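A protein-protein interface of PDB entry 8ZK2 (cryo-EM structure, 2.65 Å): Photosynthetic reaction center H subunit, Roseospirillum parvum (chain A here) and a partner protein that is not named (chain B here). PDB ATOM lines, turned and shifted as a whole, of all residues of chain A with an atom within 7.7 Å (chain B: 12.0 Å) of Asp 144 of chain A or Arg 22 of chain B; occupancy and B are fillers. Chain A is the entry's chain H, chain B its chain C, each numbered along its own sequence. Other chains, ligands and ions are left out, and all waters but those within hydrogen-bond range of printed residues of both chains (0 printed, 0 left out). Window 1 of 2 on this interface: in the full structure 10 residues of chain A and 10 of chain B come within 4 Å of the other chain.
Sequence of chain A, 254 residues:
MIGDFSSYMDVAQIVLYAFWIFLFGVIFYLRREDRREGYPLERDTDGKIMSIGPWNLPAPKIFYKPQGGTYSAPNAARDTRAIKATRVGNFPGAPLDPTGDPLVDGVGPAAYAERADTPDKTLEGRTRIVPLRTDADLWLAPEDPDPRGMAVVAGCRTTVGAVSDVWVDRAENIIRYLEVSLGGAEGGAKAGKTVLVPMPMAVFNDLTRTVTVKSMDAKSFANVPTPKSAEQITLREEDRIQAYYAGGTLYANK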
ATOM      1  N   LEU A 140      -9.034  16.522   0.826  1.00  0.00           N
ATOM      2  CA  LEU A 140      -9.701  15.263   1.121  1.00  0.00           C
ATOM      3  C   LEU A 140      -8.892  14.508   2.165  1.00  0.00           C
ATOM      4  O   LEU A 140      -7.659  14.466   2.088  1.00  0.00           O
ATOM      5  CB  LEU A 140      -9.862  14.420  -0.145  1.00  0.00           C
ATOM      6  CG  LEU A 140     -10.984  14.853  -1.089  1.00  0.00           C
ATOM      7  CD1 LEU A 140     -11.245  13.786  -2.133  1.00  0.00           C
ATOM      8  CD2 LEU A 140     -12.253  15.164  -0.312  1.00  0.00           C
ATOM      9  N   ALA A 141      -9.584  13.925   3.140  1.00  0.00           N
ATOM     10  CA  ALA A 141      -8.930  13.185   4.211  1.00  0.00           C
ATOM     11  C   ALA A 141      -8.133  12.026   3.627  1.00  0.00           C
ATOM     12  O   ALA A 141      -8.667  11.246   2.828  1.00  0.00           O
ATOM     13  CB  ALA A 141      -9.956  12.675   5.223  1.00  0.00           C
ATOM     14  N   PRO A 142      -6.854  11.886   3.988  1.00  0.00           N
ATOM     15  CA  PRO A 142      -6.047  10.788   3.434  1.00  0.00           C
ATOM     16  C   PRO A 142      -6.540   9.407   3.828  1.00  0.00           C
ATOM     17  O   PRO A 142      -6.199   8.433   3.145  1.00  0.00           O
ATOM     18  CB  PRO A 142      -4.648  11.061   4.001  1.00  0.00           C
ATOM     19  CG  PRO A 142      -4.895  11.853   5.241  1.00  0.00           C
ATOM     20  CD  PRO A 142      -6.092  12.707   4.943  1.00  0.00           C
ATOM     21  N   GLU A 143      -7.323   9.288   4.902  1.00  0.00           N
ATOM     22  CA  GLU A 143      -7.862   7.996   5.300  1.00  0.00           C
ATOM     23  C   GLU A 143      -8.932   7.486   4.345  1.00  0.00           C
ATOM     24  O   GLU A 143      -9.197   6.280   4.321  1.00  0.00           O
ATOM     25  CB  GLU A 143      -8.435   8.076   6.717  1.00  0.00           C
ATOM     26  CG  GLU A 143      -7.394   8.298   7.803  1.00  0.00           C
ATOM     27  CD  GLU A 143      -7.074   9.764   8.022  1.00  0.00           C
ATOM     28  OE1 GLU A 143      -7.719  10.620   7.381  1.00  0.00           O
ATOM     29  OE2 GLU A 143      -6.176  10.061   8.838  1.00  0.00           O
ATOM     30  N   ASP A 144      -9.548   8.370   3.561  1.00  0.00           N
ATOM     31  CA  ASP A 144     -10.591   7.952   2.641  1.00  0.00           C
ATOM     32  C   ASP A 144     -10.076   7.956   1.207  1.00  0.00           C
ATOM     33  O   ASP A 144      -9.177   8.729   0.864  1.00  0.00           O
ATOM     34  CB  ASP A 144     -11.807   8.876   2.748  1.00  0.00           C
ATOM     35  CG  ASP A 144     -12.568   8.689   4.045  1.00  0.00           C
ATOM     36  OD1 ASP A 144     -12.335   7.669   4.726  1.00  0.00           O
ATOM     37  OD2 ASP A 144     -13.394   9.560   4.387  1.00  0.00           O
ATOM     38  N   PRO A 145     -10.621   7.092   0.351  1.00  0.00           N
ATOM     39  CA  PRO A 145     -10.206   7.092  -1.056  1.00  0.00           C
ATOM     40  C   PRO A 145     -10.579   8.394  -1.745  1.00  0.00           C
ATOM     41  O   PRO A 145     -11.562   9.051  -1.397  1.00  0.00           O
ATOM     42  CB  PRO A 145     -10.971   5.906  -1.655  1.00  0.00           C
ATOM     43  CG  PRO A 145     -12.096   5.649  -0.707  1.00  0.00           C
ATOM     44  CD  PRO A 145     -11.578   6.013   0.646  1.00  0.00           C
ATOM     45  N   ASP A 146      -9.775   8.763  -2.734  1.00  0.00           N
ATOM     46  CA  ASP A 146     -10.043   9.969  -3.504  1.00  0.00           C
ATOM     47  C   ASP A 146     -10.934   9.619  -4.690  1.00  0.00           C
ATOM     48  O   ASP A 146     -10.517   8.841  -5.554  1.00  0.00           O
ATOM     49  CB  ASP A 146      -8.738  10.594  -3.984  1.00  0.00           C
ATOM     50  CG  ASP A 146      -8.912  12.027  -4.445  1.00  0.00           C
ATOM     51  OD1 ASP A 146      -9.784  12.282  -5.299  1.00  0.00           O
ATOM     52  OD2 ASP A 146      -8.172  12.904  -3.955  1.00  0.00           O
ATOM     53  N   PRO A 147     -12.158  10.149  -4.762  1.00  0.00           N
ATOM     54  CA  PRO A 147     -13.034   9.823  -5.898  1.00  0.00           C
ATOM     55  C   PRO A 147     -12.485  10.258  -7.244  1.00  0.00           C
ATOM     56  O   PRO A 147     -12.848   9.660  -8.263  1.00  0.00           O
ATOM     57  CB  PRO A 147     -14.331  10.570  -5.562  1.00  0.00           C
ATOM     58  CG  PRO A 147     -14.293  10.731  -4.080  1.00  0.00           C
ATOM     59  CD  PRO A 147     -12.851  10.969  -3.758  1.00  0.00           C
ATOM     60  N   MET A 150     -11.631   8.087 -10.684  1.00  0.00           N
ATOM     61  CA  MET A 150     -12.367   6.834 -10.736  1.00  0.00           C
ATOM     62  C   MET A 150     -13.265   6.790 -11.965  1.00  0.00           C
ATOM     63  O   MET A 150     -13.818   7.804 -12.397  1.00  0.00           O
ATOM     64  CB  MET A 150     -13.211   6.661  -9.473  1.00  0.00           C
ATOM     65  CG  MET A 150     -12.471   6.070  -8.288  1.00  0.00           C
ATOM     66  SD  MET A 150     -13.481   6.097  -6.797  1.00  0.00           S
ATOM     67  CE  MET A 150     -12.560   4.991  -5.734  1.00  0.00           C
ATOM     68  N   ILE A 175     -18.639  16.097   0.783  1.00  0.00           N
ATOM     69  CA  ILE A 175     -18.725  16.067  -0.673  1.00  0.00           C
ATOM     70  C   ILE A 175     -20.196  15.945  -1.056  1.00  0.00           C
ATOM     71  O   ILE A 175     -20.860  14.968  -0.705  1.00  0.00           O
ATOM     72  CB  ILE A 175     -17.898  14.923  -1.266  1.00  0.00           C
ATOM     73  CG1 ILE A 175     -16.437  15.044  -0.838  1.00  0.00           C
ATOM     74  CG2 ILE A 175     -18.009  14.915  -2.781  1.00  0.00           C
ATOM     75  CD1 ILE A 175     -15.634  13.791  -1.074  1.00  0.00           C
ATOM     76  N   MET A 199     -23.606  12.661  -4.523  1.00  0.00           N
ATOM     77  CA  MET A 199     -22.863  11.614  -3.827  1.00  0.00           C
ATOM     78  C   MET A 199     -23.748  10.535  -3.206  1.00  0.00           C
ATOM     79  O   MET A 199     -23.360   9.357  -3.268  1.00  0.00           O
ATOM     80  CB  MET A 199     -21.944  12.239  -2.767  1.00  0.00           C
ATOM     81  CG  MET A 199     -21.070  11.219  -2.051  1.00  0.00           C
ATOM     82  SD  MET A 199     -19.922  11.948  -0.872  1.00  0.00           S
ATOM     83  CE  MET A 199     -19.167  10.482  -0.175  1.00  0.00           C
ATOM     84  N   PHE A 204     -19.034   3.742  -4.263  1.00  0.00           N
ATOM     85  CA  PHE A 204     -17.609   3.734  -4.556  1.00  0.00           C
ATOM     86  C   PHE A 204     -17.015   2.350  -4.326  1.00  0.00           C
ATOM     87  O   PHE A 204     -17.368   1.660  -3.365  1.00  0.00           O
ATOM     88  CB  PHE A 204     -16.875   4.760  -3.694  1.00  0.00           C
ATOM     89  CG  PHE A 204     -17.279   6.176  -3.966  1.00  0.00           C
ATOM     90  CD1 PHE A 204     -16.668   6.903  -4.972  1.00  0.00           C
ATOM     91  CD2 PHE A 204     -18.276   6.780  -3.221  1.00  0.00           C
ATOM     92  CE1 PHE A 204     -17.040   8.204  -5.225  1.00  0.00           C
ATOM     93  CE2 PHE A 204     -18.653   8.083  -3.472  1.00  0.00           C
ATOM     94  CZ  PHE A 204     -18.034   8.794  -4.475  1.00  0.00           C
ATOM     95  N   ASN A 205     -16.109   1.956  -5.216  1.00  0.00           N
ATOM     96  CA  ASN A 205     -15.342   0.719  -5.095  1.00  0.00           C
ATOM     97  C   ASN A 205     -13.873   1.076  -5.275  1.00  0.00           C
ATOM     98  O   ASN A 205     -13.421   1.312  -6.399  1.00  0.00           O
ATOM     99  CB  ASN A 205     -15.790  -0.313  -6.128  1.00  0.00           C
ATOM    100  CG  ASN A 205     -15.350  -1.718  -5.778  1.00  0.00           C
ATOM    101  OD1 ASN A 205     -14.395  -1.914  -5.030  1.00  0.00           O
ATOM    102  ND2 ASN A 205     -16.047  -2.707  -6.322  1.00  0.00           N
ATOM    103  N   ASP A 206     -13.129   1.119  -4.170  1.00  0.00           N
ATOM    104  CA  ASP A 206     -11.741   1.559  -4.221  1.00  0.00           C
ATOM    105  C   ASP A 206     -10.784   0.480  -4.711  1.00  0.00           C
ATOM    106  O   ASP A 206      -9.667   0.811  -5.123  1.00  0.00           O
ATOM    107  CB  ASP A 206     -11.299   2.053  -2.843  1.00  0.00           C
ATOM    108  CG  ASP A 206     -10.047   2.901  -2.904  1.00  0.00           C
ATOM    109  OD1 ASP A 206      -9.816   3.546  -3.948  1.00  0.00           O
ATOM    110  OD2 ASP A 206      -9.300   2.936  -1.907  1.00  0.00           O
ATOM    111  N   LEU A 207     -11.181  -0.792  -4.678  1.00  0.00           N
ATOM    112  CA  LEU A 207     -10.338  -1.851  -5.217  1.00  0.00           C
ATOM    113  C   LEU A 207     -10.312  -1.862  -6.736  1.00  0.00           C
ATOM    114  O   LEU A 207      -9.244  -2.053  -7.329  1.00  0.00           O
ATOM    115  CB  LEU A 207     -10.803  -3.218  -4.710  1.00  0.00           C
ATOM    116  CG  LEU A 207     -11.114  -3.319  -3.221  1.00  0.00           C
ATOM    117  CD1 LEU A 207     -11.621  -4.712  -2.886  1.00  0.00           C
ATOM    118  CD2 LEU A 207      -9.876  -2.985  -2.406  1.00  0.00           C
ATOM    119  N   THR A 208     -11.461  -1.669  -7.380  1.00  0.00           N
ATOM    120  CA  THR A 208     -11.528  -1.591  -8.829  1.00  0.00           C
ATOM    121  C   THR A 208     -11.532  -0.163  -9.352  1.00  0.00           C
ATOM    122  O   THR A 208     -11.550   0.028 -10.572  1.00  0.00           O
ATOM    123  CB  THR A 208     -12.774  -2.324  -9.345  1.00  0.00           C
ATOM    124  OG1 THR A 208     -13.928  -1.499  -9.157  1.00  0.00           O
ATOM    125  CG2 THR A 208     -12.967  -3.628  -8.594  1.00  0.00           C
ATOM    126  N   SER B  20      -3.391   1.933   1.510  1.00  0.00           N
ATOM    127  CA  SER B  20      -3.997   0.737   0.937  1.00  0.00           C
ATOM    128  C   SER B  20      -5.458   0.984   0.578  1.00  0.00           C
ATOM    129  O   SER B  20      -6.172   1.670   1.310  1.00  0.00           O
ATOM    130  CB  SER B  20      -3.882  -0.440   1.908  1.00  0.00           C
ATOM    131  OG  SER B  20      -4.412  -0.107   3.178  1.00  0.00           O
ATOM    132  N   PRO B  21      -5.897   0.430  -0.551  1.00  0.00           N
ATOM    133  CA  PRO B  21      -7.285   0.632  -0.984  1.00  0.00           C
ATOM    134  C   PRO B  21      -8.278   0.073   0.023  1.00  0.00           C
ATOM    135  O   PRO B  21      -8.031  -0.952   0.663  1.00  0.00           O
ATOM    136  CB  PRO B  21      -7.349  -0.118  -2.320  1.00  0.00           C
ATOM    137  CG  PRO B  21      -5.924  -0.203  -2.773  1.00  0.00           C
ATOM    138  CD  PRO B  21      -5.141  -0.387  -1.513  1.00  0.00           C
ATOM    139  N   ARG B  22      -9.411   0.758   0.160  1.00  0.00           N
ATOM    140  CA  ARG B  22     -10.467   0.299   1.054  1.00  0.00           C
ATOM    141  C   ARG B  22     -11.328  -0.735   0.343  1.00  0.00           C
ATOM    142  O   ARG B  22     -11.849  -0.478  -0.747  1.00  0.00           O
ATOM    143  CB  ARG B  22     -11.316   1.476   1.526  1.00  0.00           C
ATOM    144  CG  ARG B  22     -12.104   1.186   2.792  1.00  0.00           C
ATOM    145  CD  ARG B  22     -12.881   2.398   3.277  1.00  0.00           C
ATOM    146  NE  ARG B  22     -13.917   2.806   2.336  1.00  0.00           N
ATOM    147  CZ  ARG B  22     -14.333   4.054   2.175  1.00  0.00           C
ATOM    148  NH1 ARG B  22     -13.831   5.047   2.889  1.00  0.00           N
ATOM    149  NH2 ARG B  22     -15.279   4.312   1.277  1.00  0.00           N
ATOM    150  N   ALA B  23     -11.475  -1.902   0.955  1.00  0.00           N
ATOM    151  CA  ALA B  23     -12.272  -2.969   0.367  1.00  0.00           C
ATOM    152  C   ALA B  23     -13.738  -2.786   0.735  1.00  0.00           C
ATOM    153  O   ALA B  23     -14.056  -2.667   1.924  1.00  0.00           O
ATOM    154  CB  ALA B  23     -11.775  -4.328   0.840  1.00  0.00           C
ATOM    155  N   PRO B  24     -14.652  -2.739  -0.234  1.00  0.00           N
ATOM    156  CA  PRO B  24     -16.078  -2.672   0.099  1.00  0.00           C
ATOM    157  C   PRO B  24     -16.506  -3.886   0.913  1.00  0.00           C
ATOM    158  O   PRO B  24     -16.014  -4.997   0.713  1.00  0.00           O
ATOM    159  CB  PRO B  24     -16.764  -2.640  -1.272  1.00  0.00           C
ATOM    160  CG  PRO B  24     -15.731  -3.143  -2.235  1.00  0.00           C
ATOM    161  CD  PRO B  24     -14.425  -2.682  -1.686  1.00  0.00           C
ATOM    162  N   VAL B  25     -17.431  -3.660   1.837  1.00  0.00           N
ATOM    163  CA  VAL B  25     -17.858  -4.701   2.767  1.00  0.00           C
ATOM    164  C   VAL B  25     -18.711  -5.718   2.020  1.00  0.00           C
ATOM    165  O   VAL B  25     -19.677  -5.358   1.340  1.00  0.00           O
ATOM    166  CB  VAL B  25     -18.625  -4.102   3.953  1.00  0.00           C
ATOM    167  CG1 VAL B  25     -18.851  -5.157   5.022  1.00  0.00           C
ATOM    168  CG2 VAL B  25     -17.868  -2.914   4.522  1.00  0.00           C
ATOM    169  N   TRP B  26     -18.352  -6.994   2.147  1.00  0.00           N
ATOM    170  CA  TRP B  26     -19.117  -8.083   1.555  1.00  0.00           C
ATOM    171  C   TRP B  26     -20.396  -8.316   2.346  1.00  0.00           C
ATOM    172  O   TRP B  26     -20.385  -9.028   3.354  1.00  0.00           O
ATOM    173  CB  TRP B  26     -18.268  -9.354   1.509  1.00  0.00           C
ATOM    174  CG  TRP B  26     -18.824 -10.433   0.641  1.00  0.00           C
ATOM    175  CD1 TRP B  26     -19.753 -10.297  -0.346  1.00  0.00           C
ATOM    176  CD2 TRP B  26     -18.479 -11.821   0.680  1.00  0.00           C
ATOM    177  NE1 TRP B  26     -20.012 -11.516  -0.923  1.00  0.00           N
ATOM    178  CE2 TRP B  26     -19.243 -12.469  -0.309  1.00  0.00           C
ATOM    179  CE3 TRP B  26     -17.602 -12.581   1.459  1.00  0.00           C
ATOM    180  CZ2 TRP B  26     -19.154 -13.838  -0.541  1.00  0.00           C
ATOM    181  CZ3 TRP B  26     -17.517 -13.939   1.228  1.00  0.00           C
ATOM    182  CH2 TRP B  26     -18.286 -14.553   0.235  1.00  0.00           C
ATOM    183  N   TRP B  30     -20.888 -11.474   5.062  1.00  0.00           N
ATOM    184  CA  TRP B  30     -21.130 -11.149   6.458  1.00  0.00           C
ATOM    185  C   TRP B  30     -22.538 -11.519   6.901  1.00  0.00           C
ATOM    186  O   TRP B  30     -22.751 -11.752   8.090  1.00  0.00           O
ATOM    187  CB  TRP B  30     -20.860  -9.664   6.708  1.00  0.00           C
ATOM    188  CG  TRP B  30     -19.395  -9.347   6.711  1.00  0.00           C
ATOM    189  CD1 TRP B  30     -18.709  -8.632   5.775  1.00  0.00           C
ATOM    190  CD2 TRP B  30     -18.432  -9.757   7.687  1.00  0.00           C
ATOM    191  NE1 TRP B  30     -17.380  -8.563   6.112  1.00  0.00           N
ATOM    192  CE2 TRP B  30     -17.184  -9.247   7.283  1.00  0.00           C
ATOM    193  CE3 TRP B  30     -18.506 -10.502   8.867  1.00  0.00           C
ATOM    194  CZ2 TRP B  30     -16.020  -9.456   8.015  1.00  0.00           C
ATOM    195  CZ3 TRP B  30     -17.349 -10.709   9.593  1.00  0.00           C
ATOM    196  CH2 TRP B  30     -16.123 -10.187   9.166  1.00  0.00           C
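OD1 of Asn 205 of chain A lies close to N of Leu 207 of chain A (3.4 Å).
Of the printed residues of chain B, Asp 144 of chain A touches Arg 22 (3.5 Å). Arg 22 of chain B touches just these residues of chain A: Asp 144, Pro 145, Asp 206 and Leu 207. No residue of chain B comes within 4 Å of Leu 140 of chain A. Glu 143 of chain A touches none of the printed residues of chain B. Of chain B, only Arg 22 (3.3 Å) comes within 4 Å of Pro 145 of chain A. No residue of chain B comes within 4 Å of Asp 146 of chain A. Of chain B, only Pro 21 (3.8 Å), Arg 22 (3.6 Å), Ala 23 (3.7 Å) and Pro 24 (3.7 Å) come within 4 Å of Leu 207 of chain A. Printed residues of chain A within 4 Å of Pro 24 of chain B: Asn 205 and Leu 207. Of the printed residues of chain A, Ala 23 of chain B touches Leu 207 (3.7 Å). Printed residues of chain A within 4 Å of Pro 21 of chain B: Asp 206 (3.2 Å) and Leu 207 (3.8 Å). Thr 208 of chain A touches none of the printed residues of chain B. Pro 147 of chain A touches none of the printed residues of chain B. The nearest printed residue of chain A that does not touch Ala 23 of chain B is Asp 206 of chain A (5.5 Å).
OD2 of Asp 206 of chain A lies within hydrogen-bond range of N of Arg 22 of chain B (3.0 Å). OD1 of Asp 144 of chain A is in salt-bridge range of NH1 of Arg 22 of chain B (3.5 Å).
Of the 16 printed residues of chain A, 5 touch a printed residue of chain B. Hydrophobic or aromatic side chains of chain A that line the printed part of chain B: Pro 145 and Leu 207. Along chain A the printed residues that touch a printed residue of chain B span positions 144 to 207. Along chain B the printed residues that touch a printed residue of chain A span positions 21 to 24. Among the printed residues, 9 pairs touch across the chains.
Among the printed residues, merely in contact across the chains: Asp 206 of chain A with Pro 21 of chain B, Pro 145 of chain A with Arg 22 of chain B, Asn 205 of chain A with Pro 24 of chain B, Leu 207 of chain A with Arg 22 of chain B, Leu 207 of chain A with Pro 24 of chain B, Leu 207 of chain A with Ala 23 of chain B and Leu 207 of chain A with Pro 21 of chain B.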
